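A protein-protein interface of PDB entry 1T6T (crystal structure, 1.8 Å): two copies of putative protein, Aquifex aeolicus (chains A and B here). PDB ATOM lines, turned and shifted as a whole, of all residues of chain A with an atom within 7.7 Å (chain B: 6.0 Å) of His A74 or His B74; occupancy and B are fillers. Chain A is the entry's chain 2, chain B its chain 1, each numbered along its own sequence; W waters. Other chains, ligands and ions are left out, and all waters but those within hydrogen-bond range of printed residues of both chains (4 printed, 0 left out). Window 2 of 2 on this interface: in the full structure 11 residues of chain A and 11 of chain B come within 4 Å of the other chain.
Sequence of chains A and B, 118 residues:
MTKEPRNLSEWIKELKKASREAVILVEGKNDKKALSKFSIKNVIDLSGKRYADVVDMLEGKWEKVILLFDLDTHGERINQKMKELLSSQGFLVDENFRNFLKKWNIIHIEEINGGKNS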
ATOM      1  N   GLU A  27       3.096   7.082  -7.572  1.00  0.00           N
ATOM      2  CA  GLU A  27       4.285   6.709  -6.831  1.00  0.00           C
ATOM      3  C   GLU A  27       5.093   5.598  -7.480  1.00  0.00           C
ATOM      4  O   GLU A  27       6.297   5.737  -7.675  1.00  0.00           O
ATOM      5  CB  GLU A  27       3.887   6.272  -5.421  1.00  0.00           C
ATOM      6  CG  GLU A  27       4.851   6.704  -4.334  1.00  0.00           C
ATOM      7  CD  GLU A  27       6.266   6.241  -4.582  1.00  0.00           C
ATOM      8  OE1 GLU A  27       6.506   5.013  -4.575  1.00  0.00           O
ATOM      9  OE2 GLU A  27       7.137   7.113  -4.787  1.00  0.00           O
ATOM     10  N   GLY A  28       4.431   4.498  -7.820  1.00  0.00           N
ATOM     11  CA  GLY A  28       5.157   3.370  -8.376  1.00  0.00           C
ATOM     12  C   GLY A  28       4.907   2.896  -9.789  1.00  0.00           C
ATOM     13  O   GLY A  28       3.918   3.243 -10.436  1.00  0.00           O
ATOM     14  N   ASP A  31       1.678   1.231 -10.303  1.00  0.00           N
ATOM     15  CA  ASP A  31       0.526   2.121 -10.399  1.00  0.00           C
ATOM     16  C   ASP A  31       0.432   2.543 -11.861  1.00  0.00           C
ATOM     17  O   ASP A  31      -0.652   2.625 -12.429  1.00  0.00           O
ATOM     18  CB  ASP A  31       0.706   3.365  -9.527  1.00  0.00           C
ATOM     19  CG  ASP A  31       0.841   3.033  -8.056  1.00  0.00           C
ATOM     20  OD1 ASP A  31       0.171   2.083  -7.603  1.00  0.00           O
ATOM     21  OD2 ASP A  31       1.604   3.724  -7.350  1.00  0.00           O
ATOM     22  N   SER A  47       8.884   6.975  -7.855  1.00  0.00           N
ATOM     23  CA  SER A  47       9.954   6.162  -7.282  1.00  0.00           C
ATOM     24  C   SER A  47      11.122   6.041  -8.252  1.00  0.00           C
ATOM     25  O   SER A  47      10.935   5.744  -9.432  1.00  0.00           O
ATOM     26  CB  SER A  47       9.439   4.768  -6.916  1.00  0.00           C
ATOM     27  OG  SER A  47      10.463   4.016  -6.280  1.00  0.00           O
ATOM     28  N   PHE A  69      -1.585   9.946  -5.907  1.00  0.00           N
ATOM     29  CA  PHE A  69      -0.861   9.124  -4.951  1.00  0.00           C
ATOM     30  C   PHE A  69      -1.871   8.381  -4.089  1.00  0.00           C
ATOM     31  O   PHE A  69      -3.024   8.802  -3.969  1.00  0.00           O
ATOM     32  CB  PHE A  69       0.048  10.008  -4.107  1.00  0.00           C
ATOM     33  CG  PHE A  69       1.107  10.687  -4.910  1.00  0.00           C
ATOM     34  CD1 PHE A  69       2.167   9.955  -5.438  1.00  0.00           C
ATOM     35  CD2 PHE A  69       1.017  12.043  -5.199  1.00  0.00           C
ATOM     36  CE1 PHE A  69       3.118  10.566  -6.248  1.00  0.00           C
ATOM     37  CE2 PHE A  69       1.966  12.663  -6.008  1.00  0.00           C
ATOM     38  CZ  PHE A  69       3.017  11.924  -6.534  1.00  0.00           C
ATOM     39  N   ASP A  70      -1.447   7.265  -3.505  1.00  0.00           N
ATOM     40  CA  ASP A  70      -2.340   6.472  -2.673  1.00  0.00           C
ATOM     41  C   ASP A  70      -2.932   7.295  -1.539  1.00  0.00           C
ATOM     42  O   ASP A  70      -2.388   8.327  -1.159  1.00  0.00           O
ATOM     43  CB  ASP A  70      -1.610   5.248  -2.120  1.00  0.00           C
ATOM     44  CG  ASP A  70      -1.110   4.327  -3.221  1.00  0.00           C
ATOM     45  OD1 ASP A  70      -1.664   4.377  -4.339  1.00  0.00           O
ATOM     46  OD2 ASP A  70      -0.171   3.546  -2.967  1.00  0.00           O
ATOM     47  N   LEU A  71      -4.057   6.825  -1.011  1.00  0.00           N
ATOM     48  CA  LEU A  71      -4.756   7.526   0.053  1.00  0.00           C
ATOM     49  C   LEU A  71      -4.328   7.133   1.460  1.00  0.00           C
ATOM     50  O   LEU A  71      -5.041   7.402   2.419  1.00  0.00           O
ATOM     51  CB  LEU A  71      -6.268   7.330  -0.103  1.00  0.00           C
ATOM     52  CG  LEU A  71      -6.880   7.951  -1.364  1.00  0.00           C
ATOM     53  CD1 LEU A  71      -8.360   7.633  -1.434  1.00  0.00           C
ATOM     54  CD2 LEU A  71      -6.665   9.455  -1.349  1.00  0.00           C
ATOM     55  N   ASP A  72      -3.167   6.502   1.584  1.00  0.00           N
ATOM     56  CA  ASP A  72      -2.669   6.116   2.897  1.00  0.00           C
ATOM     57  C   ASP A  72      -1.708   7.203   3.380  1.00  0.00           C
ATOM     58  O   ASP A  72      -1.466   8.180   2.671  1.00  0.00           O
ATOM     59  CB  ASP A  72      -1.978   4.746   2.824  1.00  0.00           C
ATOM     60  CG  ASP A  72      -0.752   4.746   1.937  1.00  0.00           C
ATOM     61  OD1 ASP A  72      -0.634   5.627   1.062  1.00  0.00           O
ATOM     62  OD2 ASP A  72       0.097   3.845   2.109  1.00  0.00           O
ATOM     63  N   THR A  73      -1.172   7.047   4.586  1.00  0.00           N
ATOM     64  CA  THR A  73      -0.259   8.044   5.138  1.00  0.00           C
ATOM     65  C   THR A  73       0.926   8.328   4.225  1.00  0.00           C
ATOM     66  O   THR A  73       1.288   9.484   4.004  1.00  0.00           O
ATOM     67  CB  THR A  73       0.279   7.606   6.510  1.00  0.00           C
ATOM     68  OG1 THR A  73      -0.819   7.392   7.401  1.00  0.00           O
ATOM     69  CG2 THR A  73       1.192   8.679   7.092  1.00  0.00           C
ATOM     70  N   HIS A  74       1.532   7.267   3.707  1.00  0.00           N
ATOM     71  CA  HIS A  74       2.682   7.387   2.822  1.00  0.00           C
ATOM     72  C   HIS A  74       2.328   8.204   1.578  1.00  0.00           C
ATOM     73  O   HIS A  74       3.085   9.081   1.164  1.00  0.00           O
ATOM     74  CB  HIS A  74       3.168   5.986   2.436  1.00  0.00           C
ATOM     75  CG  HIS A  74       4.356   5.979   1.525  1.00  0.00           C
ATOM     76  ND1 HIS A  74       4.244   6.042   0.153  1.00  0.00           N
ATOM     77  CD2 HIS A  74       5.682   5.907   1.792  1.00  0.00           C
ATOM     78  CE1 HIS A  74       5.450   6.008  -0.387  1.00  0.00           C
ATOM     79  NE2 HIS A  74       6.340   5.927   0.585  1.00  0.00           N
ATOM     80  N   GLY A  75       1.170   7.915   0.994  1.00  0.00           N
ATOM     81  CA  GLY A  75       0.746   8.633  -0.195  1.00  0.00           C
ATOM     82  C   GLY A  75       0.382  10.085   0.065  1.00  0.00           C
ATOM     83  O   GLY A  75       0.638  10.953  -0.770  1.00  0.00           O
ATOM     84  N   GLU A  76      -0.218  10.357   1.218  1.00  0.00           N
ATOM     85  CA  GLU A  76      -0.615  11.715   1.567  1.00  0.00           C
ATOM     86  C   GLU A  76       0.601  12.620   1.764  1.00  0.00           C
ATOM     87  O   GLU A  76       0.570  13.794   1.399  1.00  0.00           O
ATOM     88  CB  GLU A  76      -1.481  11.696   2.829  1.00  0.00           C
ATOM     89  CG  GLU A  76      -2.135  13.030   3.175  1.00  0.00           C
ATOM     90  CD  GLU A  76      -3.006  13.581   2.053  1.00  0.00           C
ATOM     91  OE1 GLU A  76      -3.771  12.803   1.444  1.00  0.00           O
ATOM     92  OE2 GLU A  76      -2.934  14.800   1.790  1.00  0.00           O
ATOM     93  N   ARG A  77       1.670  12.082   2.347  1.00  0.00           N
ATOM     94  CA  ARG A  77       2.884  12.867   2.551  1.00  0.00           C
ATOM     95  C   ARG A  77       3.498  13.226   1.201  1.00  0.00           C
ATOM     96  O   ARG A  77       3.912  14.366   0.976  1.00  0.00           O
ATOM     97  CB  ARG A  77       3.897  12.078   3.382  1.00  0.00           C
ATOM     98  CG  ARG A  77       3.464  11.858   4.816  1.00  0.00           C
ATOM     99  CD  ARG A  77       4.395  10.893   5.525  1.00  0.00           C
ATOM    100  NE  ARG A  77       4.063  10.770   6.941  1.00  0.00           N
ATOM    101  CZ  ARG A  77       4.561   9.838   7.745  1.00  0.00           C
ATOM    102  NH1 ARG A  77       5.415   8.942   7.272  1.00  0.00           N
ATOM    103  NH2 ARG A  77       4.209   9.807   9.025  1.00  0.00           N
ATOM    104  N   ILE A  78       3.555  12.253   0.298  1.00  0.00           N
ATOM    105  CA  ILE A  78       4.115  12.499  -1.025  1.00  0.00           C
ATOM    106  C   ILE A  78       3.219  13.475  -1.788  1.00  0.00           C
ATOM    107  O   ILE A  78       3.705  14.372  -2.477  1.00  0.00           O
ATOM    108  CB  ILE A  78       4.247  11.192  -1.835  1.00  0.00           C
ATOM    109  CG1 ILE A  78       5.209  10.244  -1.122  1.00  0.00           C
ATOM    110  CG2 ILE A  78       4.761  11.494  -3.239  1.00  0.00           C
ATOM    111  CD1 ILE A  78       5.408   8.923  -1.836  1.00  0.00           C
ATOM    112  N   ASN A  79       1.908  13.298  -1.656  1.00  0.00           N
ATOM    113  CA  ASN A  79       0.969  14.179  -2.331  1.00  0.00           C
ATOM    114  C   ASN A  79       1.221  15.627  -1.922  1.00  0.00           C
ATOM    115  O   ASN A  79       1.315  16.510  -2.768  1.00  0.00           O
ATOM    116  CB  ASN A  79      -0.472  13.811  -1.978  1.00  0.00           C
ATOM    117  CG  ASN A  79      -1.484  14.571  -2.814  1.00  0.00           C
ATOM    118  OD1 ASN A  79      -1.670  14.282  -3.993  1.00  0.00           O
ATOM    119  ND2 ASN A  79      -2.132  15.560  -2.208  1.00  0.00           N
ATOM    120  N   GLN A  80       1.328  15.862  -0.618  1.00  0.00           N
ATOM    121  CA  GLN A  80       1.552  17.211  -0.108  1.00  0.00           C
ATOM    122  C   GLN A  80       2.877  17.790  -0.571  1.00  0.00           C
ATOM    123  O   GLN A  80       2.955  18.959  -0.953  1.00  0.00           O
ATOM    124  CB  GLN A  80       1.493  17.221   1.420  1.00  0.00           C
ATOM    125  CG  GLN A  80       0.113  16.915   1.972  1.00  0.00           C
ATOM    126  CD  GLN A  80      -0.969  17.747   1.300  1.00  0.00           C
ATOM    127  OE1 GLN A  80      -0.898  18.978   1.273  1.00  0.00           O
ATOM    128  NE2 GLN A  80      -1.975  17.073   0.749  1.00  0.00           N
ATOM    129  N   ARG A  98      -8.028  12.496  -7.334  1.00  0.00           N
ATOM    130  CA  ARG A  98      -7.633  11.806  -6.120  1.00  0.00           C
ATOM    131  C   ARG A  98      -8.685  12.026  -5.033  1.00  0.00           C
ATOM    132  O   ARG A  98      -9.069  11.091  -4.334  1.00  0.00           O
ATOM    133  CB  ARG A  98      -6.271  12.319  -5.640  1.00  0.00           C
ATOM    134  CG  ARG A  98      -5.757  11.623  -4.386  1.00  0.00           C
ATOM    135  CD  ARG A  98      -4.304  11.989  -4.117  1.00  0.00           C
ATOM    136  NE  ARG A  98      -3.753  11.289  -2.956  1.00  0.00           N
ATOM    137  CZ  ARG A  98      -3.841  11.723  -1.704  1.00  0.00           C
ATOM    138  NH1 ARG A  98      -4.460  12.864  -1.437  1.00  0.00           N
ATOM    139  NH2 ARG A  98      -3.300  11.019  -0.717  1.00  0.00           N
ATOM    140  N   HIS A 108      -5.109   2.235  -2.527  1.00  0.00           N
ATOM    141  CA  HIS A 108      -4.013   2.172  -3.490  1.00  0.00           C
ATOM    142  C   HIS A 108      -4.536   2.223  -4.917  1.00  0.00           C
ATOM    143  O   HIS A 108      -5.432   1.464  -5.283  1.00  0.00           O
ATOM    144  CB  HIS A 108      -3.223   0.882  -3.273  1.00  0.00           C
ATOM    145  CG  HIS A 108      -2.706   0.720  -1.880  1.00  0.00           C
ATOM    146  ND1 HIS A 108      -1.664   1.470  -1.381  1.00  0.00           N
ATOM    147  CD2 HIS A 108      -3.109  -0.085  -0.867  1.00  0.00           C
ATOM    148  CE1 HIS A 108      -1.444   1.135  -0.122  1.00  0.00           C
ATOM    149  NE2 HIS A 108      -2.308   0.194   0.215  1.00  0.00           N
ATOM    150  N   GLU A 110      -3.325   1.105  -7.381  1.00  0.00           N
ATOM    151  CA  GLU A 110      -3.113  -0.205  -7.979  1.00  0.00           C
ATOM    152  C   GLU A 110      -4.365  -1.080  -7.882  1.00  0.00           C
ATOM    153  O   GLU A 110      -4.521  -2.037  -8.637  1.00  0.00           O
ATOM    154  CB  GLU A 110      -1.938  -0.901  -7.286  1.00  0.00           C
ATOM    155  CG  GLU A 110      -1.235  -1.928  -8.147  1.00  0.00           C
ATOM    156  CD  GLU A 110      -0.071  -2.580  -7.433  1.00  0.00           C
ATOM    157  OE1 GLU A 110       0.655  -1.867  -6.706  1.00  0.00           O
ATOM    158  OE2 GLU A 110       0.128  -3.800  -7.609  1.00  0.00           O
ATOM    159  N   GLU B  27      13.030   4.004   3.378  1.00  0.00           N
ATOM    160  CA  GLU B  27      12.220   4.613   2.332  1.00  0.00           C
ATOM    161  C   GLU B  27      11.983   6.104   2.522  1.00  0.00           C
ATOM    162  O   GLU B  27      12.219   6.896   1.610  1.00  0.00           O
ATOM    163  CB  GLU B  27      10.872   3.890   2.252  1.00  0.00           C
ATOM    164  CG  GLU B  27      10.043   4.179   1.005  1.00  0.00           C
ATOM    165  CD  GLU B  27       9.463   5.581   0.965  1.00  0.00           C
ATOM    166  OE1 GLU B  27       8.893   6.028   1.985  1.00  0.00           O
ATOM    167  OE2 GLU B  27       9.563   6.234  -0.095  1.00  0.00           O
ATOM    168  N   SER B  47      13.319   8.065  -0.783  1.00  0.00           N
ATOM    169  CA  SER B  47      12.358   8.941  -1.436  1.00  0.00           C
ATOM    170  C   SER B  47      13.010  10.265  -1.812  1.00  0.00           C
ATOM    171  O   SER B  47      13.644  10.909  -0.980  1.00  0.00           O
ATOM    172  CB  SER B  47      11.152   9.189  -0.525  1.00  0.00           C
ATOM    173  OG  SER B  47      10.156   9.928  -1.208  1.00  0.00           O
ATOM    174  N   ASP B  70      10.067  -0.982   4.809  1.00  0.00           N
ATOM    175  CA  ASP B  70       8.902  -1.556   5.469  1.00  0.00           C
ATOM    176  C   ASP B  70       8.571  -2.922   4.888  1.00  0.00           C
ATOM    177  O   ASP B  70       8.987  -3.253   3.779  1.00  0.00           O
ATOM    178  CB  ASP B  70       7.696  -0.616   5.352  1.00  0.00           C
ATOM    179  CG  ASP B  70       7.879   0.666   6.145  1.00  0.00           C
ATOM    180  OD1 ASP B  70       8.784   0.706   7.009  1.00  0.00           O
ATOM    181  OD2 ASP B  70       7.117   1.630   5.916  1.00  0.00           O
ATOM    182  N   ASP B  72       5.581  -3.975   4.099  1.00  0.00           N
ATOM    183  CA  ASP B  72       4.384  -3.973   3.266  1.00  0.00           C
ATOM    184  C   ASP B  72       4.785  -4.250   1.818  1.00  0.00           C
ATOM    185  O   ASP B  72       5.965  -4.426   1.518  1.00  0.00           O
ATOM    186  CB  ASP B  72       3.637  -2.635   3.369  1.00  0.00           C
ATOM    187  CG  ASP B  72       4.517  -1.439   3.064  1.00  0.00           C
ATOM    188  OD1 ASP B  72       5.511  -1.594   2.326  1.00  0.00           O
ATOM    189  OD2 ASP B  72       4.201  -0.332   3.551  1.00  0.00           O
ATOM    190  N   THR B  73       3.803  -4.298   0.923  1.00  0.00           N
ATOM    191  CA  THR B  73       4.074  -4.570  -0.482  1.00  0.00           C
ATOM    192  C   THR B  73       4.984  -3.520  -1.102  1.00  0.00           C
ATOM    193  O   THR B  73       5.915  -3.851  -1.836  1.00  0.00           O
ATOM    194  CB  THR B  73       2.767  -4.641  -1.293  1.00  0.00           C
ATOM    195  OG1 THR B  73       1.950  -5.697  -0.774  1.00  0.00           O
ATOM    196  CG2 THR B  73       3.061  -4.911  -2.763  1.00  0.00           C
ATOM    197  N   HIS B  74       4.707  -2.254  -0.808  1.00  0.00           N
ATOM    198  CA  HIS B  74       5.508  -1.156  -1.330  1.00  0.00           C
ATOM    199  C   HIS B  74       6.962  -1.338  -0.888  1.00  0.00           C
ATOM    200  O   HIS B  74       7.888  -1.224  -1.693  1.00  0.00           O
ATOM    201  CB  HIS B  74       4.963   0.179  -0.808  1.00  0.00           C
ATOM    202  CG  HIS B  74       5.791   1.366  -1.190  1.00  0.00           C
ATOM    203  ND1 HIS B  74       5.878   1.831  -2.484  1.00  0.00           N
ATOM    204  CD2 HIS B  74       6.582   2.176  -0.446  1.00  0.00           C
ATOM    205  CE1 HIS B  74       6.687   2.874  -2.523  1.00  0.00           C
ATOM    206  NE2 HIS B  74       7.129   3.105  -1.300  1.00  0.00           N
ATOM    207  N   GLY B  75       7.147  -1.635   0.397  1.00  0.00           N
ATOM    208  CA  GLY B  75       8.479  -1.822   0.946  1.00  0.00           C
ATOM    209  C   GLY B  75       9.241  -3.012   0.390  1.00  0.00           C
ATOM    210  O   GLY B  75      10.440  -2.916   0.132  1.00  0.00           O
ATOM    211  N   GLU B  76       8.552  -4.134   0.206  1.00  0.00           N
ATOM    212  CA  GLU B  76       9.180  -5.344  -0.318  1.00  0.00           C
ATOM    213  C   GLU B  76       9.672  -5.138  -1.750  1.00  0.00           C
ATOM    214  O   GLU B  76      10.727  -5.643  -2.132  1.00  0.00           O
ATOM    215  CB  GLU B  76       8.190  -6.510  -0.274  1.00  0.00           C
ATOM    216  CG  GLU B  76       8.803  -7.869  -0.577  1.00  0.00           C
ATOM    217  CD  GLU B  76       9.972  -8.201   0.337  1.00  0.00           C
ATOM    218  OE1 GLU B  76       9.900  -7.878   1.542  1.00  0.00           O
ATOM    219  OE2 GLU B  76      10.958  -8.792  -0.149  1.00  0.00           O
ATOM    220  N   ARG B  77       8.901  -4.404  -2.545  1.00  0.00           N
ATOM    221  CA  ARG B  77       9.292  -4.136  -3.924  1.00  0.00           C
ATOM    222  C   ARG B  77      10.552  -3.279  -3.962  1.00  0.00           C
ATOM    223  O   ARG B  77      11.461  -3.534  -4.753  1.00  0.00           O
ATOM    224  CB  ARG B  77       8.161  -3.428  -4.663  1.00  0.00           C
ATOM    225  CG  ARG B  77       6.957  -4.312  -4.909  1.00  0.00           C
ATOM    226  CD  ARG B  77       5.794  -3.501  -5.446  1.00  0.00           C
ATOM    227  NE  ARG B  77       4.688  -4.353  -5.869  1.00  0.00           N
ATOM    228  CZ  ARG B  77       3.476  -3.900  -6.166  1.00  0.00           C
ATOM    229  NH1 ARG B  77       3.216  -2.603  -6.082  1.00  0.00           N
ATOM    230  NH2 ARG B  77       2.524  -4.743  -6.545  1.00  0.00           N
ATOM    231  N   ILE B  78      10.608  -2.262  -3.108  1.00  0.00           N
ATOM    232  CA  ILE B  78      11.778  -1.395  -3.070  1.00  0.00           C
ATOM    233  C   ILE B  78      12.969  -2.185  -2.531  1.00  0.00           C
ATOM    234  O   ILE B  78      14.094  -2.035  -3.008  1.00  0.00           O
ATOM    235  CB  ILE B  78      11.521  -0.147  -2.193  1.00  0.00           C
ATOM    236  CG1 ILE B  78      10.465   0.735  -2.866  1.00  0.00           C
ATOM    237  CG2 ILE B  78      12.812   0.644  -2.005  1.00  0.00           C
ATOM    238  CD1 ILE B  78      10.065   1.956  -2.064  1.00  0.00           C
ATOM    239  N   ASN B  79      12.715  -3.046  -1.552  1.00  0.00           N
ATOM    240  CA  ASN B  79      13.777  -3.861  -0.975  1.00  0.00           C
ATOM    241  C   ASN B  79      14.427  -4.722  -2.054  1.00  0.00           C
ATOM    242  O   ASN B  79      15.650  -4.778  -2.161  1.00  0.00           O
ATOM    243  CB  ASN B  79      13.220  -4.753   0.139  1.00  0.00           C
ATOM    244  CG  ASN B  79      14.299  -5.578   0.824  1.00  0.00           C
ATOM    245  OD1 ASN B  79      14.478  -6.762   0.530  1.00  0.00           O
ATOM    246  ND2 ASN B  79      15.033  -4.948   1.732  1.00  0.00           N
HETATM  247  O   HOH W   1       2.464   0.476  -7.341  1.00  0.00           O
HETATM  248  O   HOH W   2       9.241   6.188  -2.871  1.00  0.00           O
HETATM  249  O   HOH W   3       9.031   8.698  -3.888  1.00  0.00           O
HETATM  250  O   HOH W   4       7.477   2.421  -5.442  1.00  0.00           O
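OE1 of Glu B27 sits at hydrogen-bond distance from NE2 of His A74, 2.9 Å away.
OE1 of Glu A110 is in salt-bridge range of NH1 of Arg B77 (2.7 Å).
NE2 of His B74 sits close to NE2 of His A74 (3.5 Å).
OD1 of Asp B72 lies close to N of His B74.
O of Glu B27 lies within hydrogen-bond range of N of Ser B47 (2.9 Å).
The backbone carbonyl oxygen (O) of Glu A27 is in hydrogen-bond range of the backbone NH (N) of Ser A47, at 2.9 Å.
Among the printed residues, pairs that only touch across the chains: Glu A27 with His B74 (3.0 Å).
Of the printed residues of chain B, Glu A27 touches His B74 (3.0 Å).
Ser A47 touches none of the printed residues of chain B.
Of chain B, only Glu B27 (2.9 Å) and His B74 (3.5 Å) come within 4 Å of His A74.
Printed residues of chain B within 4 Å of Glu A110: Arg B77 (2.7 Å).
Of the printed residues of chain A, Glu B27 touches His A74.
His B74 touches just these residues of chain A: Glu A27 and His A74.
No residue of chain A comes within 4 Å of Gly B75.
The nearest residue of chain B that does not touch His A74 is Ser B47 (5.8 Å).
The nearest residue of chain A that does not touch His B74 is Ser A47 (5.4 Å).
The nearest printed residue of chain B that does not touch Glu A27 is Ile B78 (5.3 Å).
Of the 19 printed residues of chain A, 3 touch a printed residue of chain B.
Printed residues of chain A that touch a printed residue of chain B: Glu A27, His A74 and Glu A110.
Of the 11 printed residues of chain B, 3 touch a printed residue of chain A.
Hydrophobic or aromatic side chains of chain B within 4 Å of the printed part of chain A: His B74.
Among the printed residues, 4 pairs touch across the chains.
Among the printed residues, Asp or Glu carboxylates within 4 Å of a Lys or Arg side-chain nitrogen of the other chain: Glu A110 with Arg B77 (2.7 Å).
Glu A27 touches His B74, and with the chains exchanged His A74 touches Glu B27.
His B74 touches its own counterpart, His A74.
Water W3 bridges the side-chain carboxylate of Glu A27 (2.6 Å) and the side-chain hydroxyl of Ser B47 (3.2 Å).
Water W2 lies within hydrogen-bond range of OE2 of Glu B27 and OE2 of Glu A27.
Water W1 lies within hydrogen-bond range of the side-chain carboxylate (OD1) of Asp A31 (2.8 Å), the side-chain carboxylate (OE1) of Glu A110 (3.0 Å) and the guanidinium group (NH1) of Arg B77 (3.4 Å).
Water W4 lies within hydrogen-bond range of OE1 of Glu A27 (2.9 Å), ND1 of His B74 (3.4 Å) and OG of Ser A47 (3.5 Å).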
